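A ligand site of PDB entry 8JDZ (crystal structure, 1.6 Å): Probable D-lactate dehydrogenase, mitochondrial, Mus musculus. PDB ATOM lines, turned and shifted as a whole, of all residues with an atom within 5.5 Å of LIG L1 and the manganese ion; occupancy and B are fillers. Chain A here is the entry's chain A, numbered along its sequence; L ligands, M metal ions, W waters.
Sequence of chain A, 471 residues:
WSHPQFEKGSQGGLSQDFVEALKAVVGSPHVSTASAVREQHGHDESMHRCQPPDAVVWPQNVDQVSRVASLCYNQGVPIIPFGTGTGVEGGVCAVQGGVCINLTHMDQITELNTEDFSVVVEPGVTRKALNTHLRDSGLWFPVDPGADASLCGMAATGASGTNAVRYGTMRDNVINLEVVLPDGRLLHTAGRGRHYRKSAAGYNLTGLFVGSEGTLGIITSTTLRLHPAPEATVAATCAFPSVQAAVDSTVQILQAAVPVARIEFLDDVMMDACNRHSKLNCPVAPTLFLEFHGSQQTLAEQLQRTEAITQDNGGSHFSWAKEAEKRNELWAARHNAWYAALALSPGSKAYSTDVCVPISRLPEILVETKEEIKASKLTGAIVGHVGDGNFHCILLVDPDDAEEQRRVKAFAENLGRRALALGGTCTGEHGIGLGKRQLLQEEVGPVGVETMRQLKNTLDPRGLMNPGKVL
Val 88 touches LIG L1.
CE3 of Trp 338 touches C6 of LIG L1, 3.6 Å away.
CD1 of Ile 394 touches C4 of LIG L1, 3.8 Å away.
Hydrophobic or aromatic side chains within 4 Å of LIG L1: Val 88, Trp 338, His 385, His 392, Ile 394 and His 430.
Within 4 Å of LIG L1: Val 88, Arg 334, Trp 338, His 385, His 392, Ile 394, Glu 429 and His 430.
Water W2 lies within hydrogen-bond range of N of Trp 338, O3 of LIG L1, O of His 335 and N of Ala 337.
Water W1 lies within hydrogen-bond range of an oxygen (O3) of LIG L1 (2.9 Å), the guanidinium group (NH1) of Arg 334 (3.3 Å) and the backbone NH (N) of Gly 146 (3.3 Å).
An oxygen (O3) of LIG L1 lies within salt-bridge range of the guanidinium group of Arg 334 (2.9 Å).
A ring nitrogen (NE2) of His 430 lies close to an oxygen (O1) of LIG L1 (2.8 Å).
A nitrogen (N8) of LG2 L2 sits at hydrogen-bond distance from the backbone NH (N) of Gly 146 (3.0 Å).
The manganese ion is bound by the side-chain carboxylate (OE2) of Glu 429 (2.1 Å), an oxygen (O2) of LIG L1 (2.2 Å), a ring nitrogen (NE2) of His 385 (2.4 Å), a ring nitrogen (NE2) of His 392 (2.4 Å), an oxygen (O1) of LIG L1 (2.6 Å) and an oxygen (O8) of LG2 L2 (2.7 Å).
The manganese ion has six donor atoms within binding distance.
O of His 385 lies within hydrogen-bond range of N of Asn 390, at 3.3 Å.
OE2 of Glu 264 lies within hydrogen-bond range of ND1 of His 385 (2.7 Å).
The backbone NH (N) of His 392 sits at hydrogen-bond distance from the backbone carbonyl oxygen (O) of Val 383 (2.7 Å).
The side-chain carboxylate (OE1) of Glu 264 lies within salt-bridge range of the guanidinium group (NE) of Arg 334, at 2.8 Å.
Of the 17 residues printed, 3 come within 4 Å of the manganese ion.
The nearest printed residue that does not touch the manganese ion is His 430 (4.2 Å).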
ATOM      1  N   VAL A  88      17.727  14.928   5.017  1.00  0.00           N
ATOM      2  CA  VAL A  88      16.792  13.909   5.469  1.00  0.00           C
ATOM      3  C   VAL A  88      17.282  13.145   6.692  1.00  0.00           C
ATOM      4  O   VAL A  88      16.771  12.065   6.995  1.00  0.00           O
ATOM      5  CB  VAL A  88      16.440  12.928   4.327  1.00  0.00           C
ATOM      6  CG1 VAL A  88      15.706  13.653   3.194  1.00  0.00           C
ATOM      7  CG2 VAL A  88      17.655  12.218   3.792  1.00  0.00           C
ATOM      8  N   GLY A 146      17.556  14.923  -5.849  1.00  0.00           N
ATOM      9  CA  GLY A 146      16.210  15.216  -6.318  1.00  0.00           C
ATOM     10  C   GLY A 146      15.748  16.623  -5.977  1.00  0.00           C
ATOM     11  O   GLY A 146      15.041  17.265  -6.766  1.00  0.00           O
ATOM     12  N   GLY A 161      23.874  11.526  -6.577  1.00  0.00           N
ATOM     13  CA  GLY A 161      22.637  11.615  -7.336  1.00  0.00           C
ATOM     14  C   GLY A 161      22.649  10.628  -8.478  1.00  0.00           C
ATOM     15  O   GLY A 161      23.561   9.801  -8.591  1.00  0.00           O
ATOM     16  N   GLU A 264      18.985   3.882 -12.666  1.00  0.00           N
ATOM     17  CA  GLU A 264      18.151   4.021 -11.485  1.00  0.00           C
ATOM     18  C   GLU A 264      17.157   2.882 -11.379  1.00  0.00           C
ATOM     19  O   GLU A 264      16.523   2.511 -12.382  1.00  0.00           O
ATOM     20  CB  GLU A 264      17.393   5.349 -11.509  1.00  0.00           C
ATOM     21  CG  GLU A 264      18.310   6.553 -11.369  1.00  0.00           C
ATOM     22  CD  GLU A 264      18.942   6.607  -9.984  1.00  0.00           C
ATOM     23  OE1 GLU A 264      18.200   6.584  -8.983  1.00  0.00           O
ATOM     24  OE2 GLU A 264      20.188   6.717  -9.906  1.00  0.00           O
ATOM     25  N   ARG A 334      11.496  10.872 -11.395  1.00  0.00           N
ATOM     26  CA  ARG A 334      12.471  10.203 -10.546  1.00  0.00           C
ATOM     27  C   ARG A 334      12.901  11.123  -9.408  1.00  0.00           C
ATOM     28  O   ARG A 334      12.897  10.716  -8.236  1.00  0.00           O
ATOM     29  CB  ARG A 334      13.683   9.765 -11.388  1.00  0.00           C
ATOM     30  CG  ARG A 334      14.898   9.335 -10.565  1.00  0.00           C
ATOM     31  CD  ARG A 334      14.580   8.179  -9.639  1.00  0.00           C
ATOM     32  NE  ARG A 334      15.720   7.905  -8.765  1.00  0.00           N
ATOM     33  CZ  ARG A 334      15.851   8.404  -7.538  1.00  0.00           C
ATOM     34  NH1 ARG A 334      14.921   9.216  -7.023  1.00  0.00           N
ATOM     35  NH2 ARG A 334      16.939   8.115  -6.828  1.00  0.00           N
ATOM     36  N   HIS A 335      13.224  12.376  -9.734  1.00  0.00           N
ATOM     37  CA  HIS A 335      13.660  13.320  -8.719  1.00  0.00           C
ATOM     38  C   HIS A 335      12.579  13.597  -7.675  1.00  0.00           C
ATOM     39  O   HIS A 335      12.897  13.996  -6.562  1.00  0.00           O
ATOM     40  CB  HIS A 335      14.117  14.632  -9.380  1.00  0.00           C
ATOM     41  CG  HIS A 335      15.452  14.529 -10.064  1.00  0.00           C
ATOM     42  ND1 HIS A 335      15.768  15.242 -11.200  1.00  0.00           N
ATOM     43  CD2 HIS A 335      16.560  13.809  -9.754  1.00  0.00           C
ATOM     44  CE1 HIS A 335      17.008  14.959 -11.569  1.00  0.00           C
ATOM     45  NE2 HIS A 335      17.507  14.094 -10.703  1.00  0.00           N
ATOM     46  N   ALA A 337      10.501  11.202  -6.552  1.00  0.00           N
ATOM     47  CA  ALA A 337      10.104   9.924  -5.967  1.00  0.00           C
ATOM     48  C   ALA A 337       9.813  10.034  -4.472  1.00  0.00           C
ATOM     49  O   ALA A 337       8.913   9.368  -3.953  1.00  0.00           O
ATOM     50  CB  ALA A 337      11.195   8.885  -6.227  1.00  0.00           C
ATOM     51  N   TRP A 338      10.587  10.849  -3.759  1.00  0.00           N
ATOM     52  CA  TRP A 338      10.329  11.061  -2.341  1.00  0.00           C
ATOM     53  C   TRP A 338       8.897  11.528  -2.125  1.00  0.00           C
ATOM     54  O   TRP A 338       8.173  10.972  -1.294  1.00  0.00           O
ATOM     55  CB  TRP A 338      11.340  12.070  -1.800  1.00  0.00           C
ATOM     56  CG  TRP A 338      11.151  12.532  -0.381  1.00  0.00           C
ATOM     57  CD1 TRP A 338      10.664  13.743   0.028  1.00  0.00           C
ATOM     58  CD2 TRP A 338      11.500  11.819   0.799  1.00  0.00           C
ATOM     59  NE1 TRP A 338      10.697  13.824   1.401  1.00  0.00           N
ATOM     60  CE2 TRP A 338      11.212  12.649   1.899  1.00  0.00           C
ATOM     61  CE3 TRP A 338      12.041  10.548   1.041  1.00  0.00           C
ATOM     62  CZ2 TRP A 338      11.412  12.256   3.220  1.00  0.00           C
ATOM     63  CZ3 TRP A 338      12.248  10.154   2.349  1.00  0.00           C
ATOM     64  CH2 TRP A 338      11.951  11.008   3.425  1.00  0.00           C
ATOM     65  N   SER A 352      14.158   7.640   4.922  1.00  0.00           N
ATOM     66  CA  SER A 352      14.884   6.943   3.873  1.00  0.00           C
ATOM     67  C   SER A 352      16.086   6.230   4.467  1.00  0.00           C
ATOM     68  O   SER A 352      16.836   6.827   5.244  1.00  0.00           O
ATOM     69  CB  SER A 352      15.365   7.900   2.781  1.00  0.00           C
ATOM     70  OG  SER A 352      15.967   7.172   1.727  1.00  0.00           O
ATOM     71  N   VAL A 383      13.943   2.652  -4.285  1.00  0.00           N
ATOM     72  CA  VAL A 383      14.422   3.458  -5.400  1.00  0.00           C
ATOM     73  C   VAL A 383      15.896   3.716  -5.152  1.00  0.00           C
ATOM     74  O   VAL A 383      16.337   3.799  -4.004  1.00  0.00           O
ATOM     75  CB  VAL A 383      13.609   4.778  -5.516  1.00  0.00           C
ATOM     76  CG1 VAL A 383      13.834   5.685  -4.293  1.00  0.00           C
ATOM     77  CG2 VAL A 383      13.959   5.528  -6.787  1.00  0.00           C
ATOM     78  N   GLY A 384      16.670   3.840  -6.229  1.00  0.00           N
ATOM     79  CA  GLY A 384      17.933   4.554  -6.063  1.00  0.00           C
ATOM     80  C   GLY A 384      19.047   4.121  -6.999  1.00  0.00           C
ATOM     81  O   GLY A 384      18.844   3.488  -8.035  1.00  0.00           O
ATOM     82  N   HIS A 385      20.238   4.550  -6.579  1.00  0.00           N
ATOM     83  CA  HIS A 385      21.431   4.639  -7.418  1.00  0.00           C
ATOM     84  C   HIS A 385      22.175   3.305  -7.410  1.00  0.00           C
ATOM     85  O   HIS A 385      23.289   3.160  -6.904  1.00  0.00           O
ATOM     86  CB  HIS A 385      22.327   5.767  -6.914  1.00  0.00           C
ATOM     87  CG  HIS A 385      21.574   7.005  -6.522  1.00  0.00           C
ATOM     88  ND1 HIS A 385      20.747   7.681  -7.397  1.00  0.00           N
ATOM     89  CD2 HIS A 385      21.515   7.689  -5.352  1.00  0.00           C
ATOM     90  CE1 HIS A 385      20.224   8.734  -6.789  1.00  0.00           C
ATOM     91  NE2 HIS A 385      20.666   8.758  -5.541  1.00  0.00           N
ATOM     92  N   ASN A 390      24.004   1.287  -4.334  1.00  0.00           N
ATOM     93  CA  ASN A 390      23.314   2.100  -3.346  1.00  0.00           C
ATOM     94  C   ASN A 390      21.814   2.065  -3.648  1.00  0.00           C
ATOM     95  O   ASN A 390      21.412   1.986  -4.805  1.00  0.00           O
ATOM     96  CB  ASN A 390      23.929   3.535  -3.440  1.00  0.00           C
ATOM     97  CG  ASN A 390      23.227   4.603  -2.601  1.00  0.00           C
ATOM     98  OD1 ASN A 390      22.924   5.683  -3.114  1.00  0.00           O
ATOM     99  ND2 ASN A 390      23.013   4.348  -1.303  1.00  0.00           N
ATOM    100  N   HIS A 392      17.684   3.322  -1.756  1.00  0.00           N
ATOM    101  CA  HIS A 392      16.878   3.858  -0.676  1.00  0.00           C
ATOM    102  C   HIS A 392      15.635   3.007  -0.503  1.00  0.00           C
ATOM    103  O   HIS A 392      14.982   2.668  -1.489  1.00  0.00           O
ATOM    104  CB  HIS A 392      16.444   5.300  -0.925  1.00  0.00           C
ATOM    105  CG  HIS A 392      17.544   6.186  -1.392  1.00  0.00           C
ATOM    106  ND1 HIS A 392      18.636   6.508  -0.602  1.00  0.00           N
ATOM    107  CD2 HIS A 392      17.720   6.848  -2.566  1.00  0.00           C
ATOM    108  CE1 HIS A 392      19.439   7.321  -1.276  1.00  0.00           C
ATOM    109  NE2 HIS A 392      18.904   7.544  -2.471  1.00  0.00           N
ATOM    110  N   ILE A 394      12.207   3.851   1.141  1.00  0.00           N
ATOM    111  CA  ILE A 394      11.421   4.961   1.680  1.00  0.00           C
ATOM    112  C   ILE A 394      10.308   4.366   2.518  1.00  0.00           C
ATOM    113  O   ILE A 394       9.385   3.744   1.980  1.00  0.00           O
ATOM    114  CB  ILE A 394      10.842   5.849   0.562  1.00  0.00           C
ATOM    115  CG1 ILE A 394      11.973   6.434  -0.289  1.00  0.00           C
ATOM    116  CG2 ILE A 394      10.043   6.974   1.174  1.00  0.00           C
ATOM    117  CD1 ILE A 394      11.486   7.055  -1.592  1.00  0.00           C
ATOM    118  N   GLU A 429      25.130   8.589   0.714  1.00  0.00           N
ATOM    119  CA  GLU A 429      25.079   9.998   0.330  1.00  0.00           C
ATOM    120  C   GLU A 429      24.334  10.926   1.311  1.00  0.00           C
ATOM    121  O   GLU A 429      24.672  12.113   1.413  1.00  0.00           O
ATOM    122  CB  GLU A 429      24.449  10.130  -1.063  1.00  0.00           C
ATOM    123  CG  GLU A 429      23.024   9.572  -1.116  1.00  0.00           C
ATOM    124  CD  GLU A 429      22.299   9.900  -2.401  1.00  0.00           C
ATOM    125  OE1 GLU A 429      22.934  10.382  -3.361  1.00  0.00           O
ATOM    126  OE2 GLU A 429      21.077   9.692  -2.426  1.00  0.00           O
ATOM    127  N   HIS A 430      23.323  10.420   2.017  1.00  0.00           N
ATOM    128  CA  HIS A 430      22.490  11.297   2.841  1.00  0.00           C
ATOM    129  C   HIS A 430      23.226  11.801   4.082  1.00  0.00           C
ATOM    130  O   HIS A 430      22.935  12.915   4.566  1.00  0.00           O
ATOM    131  CB  HIS A 430      21.223  10.567   3.285  1.00  0.00           C
ATOM    132  CG  HIS A 430      20.244  10.389   2.186  1.00  0.00           C
ATOM    133  ND1 HIS A 430      19.209   9.475   2.262  1.00  0.00           N
ATOM    134  CD2 HIS A 430      20.126  10.997   0.979  1.00  0.00           C
ATOM    135  CE1 HIS A 430      18.504   9.523   1.143  1.00  0.00           C
ATOM    136  NE2 HIS A 430      19.047  10.433   0.346  1.00  0.00           N
HETATM  137  C1  LIG L   1      16.556  10.289  -4.099  1.00  0.00           C
HETATM  138  C2  LIG L   1      16.619  10.448  -2.584  1.00  0.00           C
HETATM  139  C3  LIG L   1      15.318  10.465  -1.800  1.00  0.00           C
HETATM  140  C4  LIG L   1      14.660   9.097  -1.884  1.00  0.00           C
HETATM  141  C5  LIG L   1      15.621  10.784  -0.343  1.00  0.00           C
HETATM  142  C6  LIG L   1      15.086  12.179  -0.046  1.00  0.00           C
HETATM  143  O1  LIG L   1      17.686  10.530  -2.053  1.00  0.00           O
HETATM  144  O2  LIG L   1      17.456   9.635  -4.670  1.00  0.00           O
HETATM  145  O3  LIG L   1      15.597  10.820  -4.744  1.00  0.00           O
HETATM  146  P1  LG2 L   2      20.267  21.272   5.003  1.00  0.00           P
HETATM  147  O1  LG2 L   2      19.125  20.381   5.385  1.00  0.00           O
HETATM  148  O2  LG2 L   2      20.117  22.768   5.022  1.00  0.00           O
HETATM  149  O3  LG2 L   2      21.529  20.890   5.865  1.00  0.00           O
HETATM  150  C1  LG2 L   2      22.047  19.542   5.836  1.00  0.00           C
HETATM  151  C2  LG2 L   2      23.199  19.395   6.801  1.00  0.00           C
HETATM  152  O4  LG2 L   2      24.355  20.080   6.278  1.00  0.00           O
HETATM  153  C3  LG2 L   2      22.972  19.970   8.199  1.00  0.00           C
HETATM  154  O5  LG2 L   2      23.640  19.190   9.182  1.00  0.00           O
HETATM  155  C4  LG2 L   2      23.521  21.389   8.082  1.00  0.00           C
HETATM  156  O6  LG2 L   2      23.983  21.922   9.317  1.00  0.00           O
HETATM  157  C5  LG2 L   2      24.684  21.192   7.103  1.00  0.00           C
HETATM  158  N1  LG2 L   2      24.939  22.322   6.242  1.00  0.00           N
HETATM  159  C6  LG2 L   2      24.115  22.878   5.292  1.00  0.00           C
HETATM  160  N2  LG2 L   2      24.661  23.857   4.614  1.00  0.00           N
HETATM  161  C7  LG2 L   2      25.940  23.956   5.164  1.00  0.00           C
HETATM  162  C8  LG2 L   2      27.019  24.808   4.881  1.00  0.00           C
HETATM  163  N3  LG2 L   2      27.004  25.755   3.953  1.00  0.00           N
HETATM  164  N4  LG2 L   2      28.144  24.634   5.615  1.00  0.00           N
HETATM  165  C9  LG2 L   2      28.181  23.670   6.543  1.00  0.00           C
HETATM  166  N5  LG2 L   2      27.213  22.807   6.887  1.00  0.00           N
HETATM  167  C10 LG2 L   2      26.115  23.015   6.149  1.00  0.00           C
HETATM  168  N6  LG2 L   2      20.601  13.836  -1.134  1.00  0.00           N
HETATM  169  C11 LG2 L   2      21.502  13.147  -1.909  1.00  0.00           C
HETATM  170  O7  LG2 L   2      22.698  13.034  -1.590  1.00  0.00           O
HETATM  171  N7  LG2 L   2      21.096  12.592  -3.098  1.00  0.00           N
HETATM  172  C12 LG2 L   2      19.802  12.611  -3.623  1.00  0.00           C
HETATM  173  O8  LG2 L   2      19.564  12.049  -4.690  1.00  0.00           O
HETATM  174  C13 LG2 L   2      18.855  13.354  -2.809  1.00  0.00           C
HETATM  175  N8  LG2 L   2      17.602  13.455  -3.227  1.00  0.00           N
HETATM  176  C14 LG2 L   2      16.705  14.138  -2.441  1.00  0.00           C
HETATM  177  C15 LG2 L   2      15.385  14.257  -2.870  1.00  0.00           C
HETATM  178  C16 LG2 L   2      14.446  14.956  -2.121  1.00  0.00           C
HETATM  179  C17 LG2 L   2      13.027  15.055  -2.616  1.00  0.00           C
HETATM  180  C18 LG2 L   2      14.825  15.544  -0.902  1.00  0.00           C
HETATM  181  C19 LG2 L   2      13.812  16.283  -0.061  1.00  0.00           C
HETATM  182  C20 LG2 L   2      16.137  15.426  -0.462  1.00  0.00           C
HETATM  183  C21 LG2 L   2      17.083  14.735  -1.225  1.00  0.00           C
HETATM  184  N9  LG2 L   2      18.421  14.618  -0.802  1.00  0.00           N
HETATM  185  C22 LG2 L   2      19.334  13.919  -1.576  1.00  0.00           C
HETATM  186  C23 LG2 L   2      18.860  15.151   0.502  1.00  0.00           C
HETATM  187  C24 LG2 L   2      19.311  16.604   0.464  1.00  0.00           C
HETATM  188  O9  LG2 L   2      18.750  17.263  -0.672  1.00  0.00           O
HETATM  189  C25 LG2 L   2      20.838  16.643   0.397  1.00  0.00           C
HETATM  190  O10 LG2 L   2      21.342  15.979   1.548  1.00  0.00           O
HETATM  191  C26 LG2 L   2      21.384  18.069   0.312  1.00  0.00           C
HETATM  192  O11 LG2 L   2      22.799  17.991   0.133  1.00  0.00           O
HETATM  193  C27 LG2 L   2      21.079  18.895   1.545  1.00  0.00           C
HETATM  194  O12 LG2 L   2      21.384  20.284   1.282  1.00  0.00           O
HETATM  195  P2  LG2 L   2      20.671  21.419   2.105  1.00  0.00           P
HETATM  196  O13 LG2 L   2      21.388  22.766   1.968  1.00  0.00           O
HETATM  197  O14 LG2 L   2      19.196  21.475   1.731  1.00  0.00           O
HETATM  198  O15 LG2 L   2      20.812  20.853   3.572  1.00  0.00           O
HETATM  199 MN    MN M   1      19.429   9.574  -3.711  1.00  0.00          MN
HETATM  200  O   HOH W   1      16.522  12.064  -7.155  1.00  0.00           O
HETATM  201  O   HOH W   2      12.998  11.924  -4.621  1.00  0.00           O
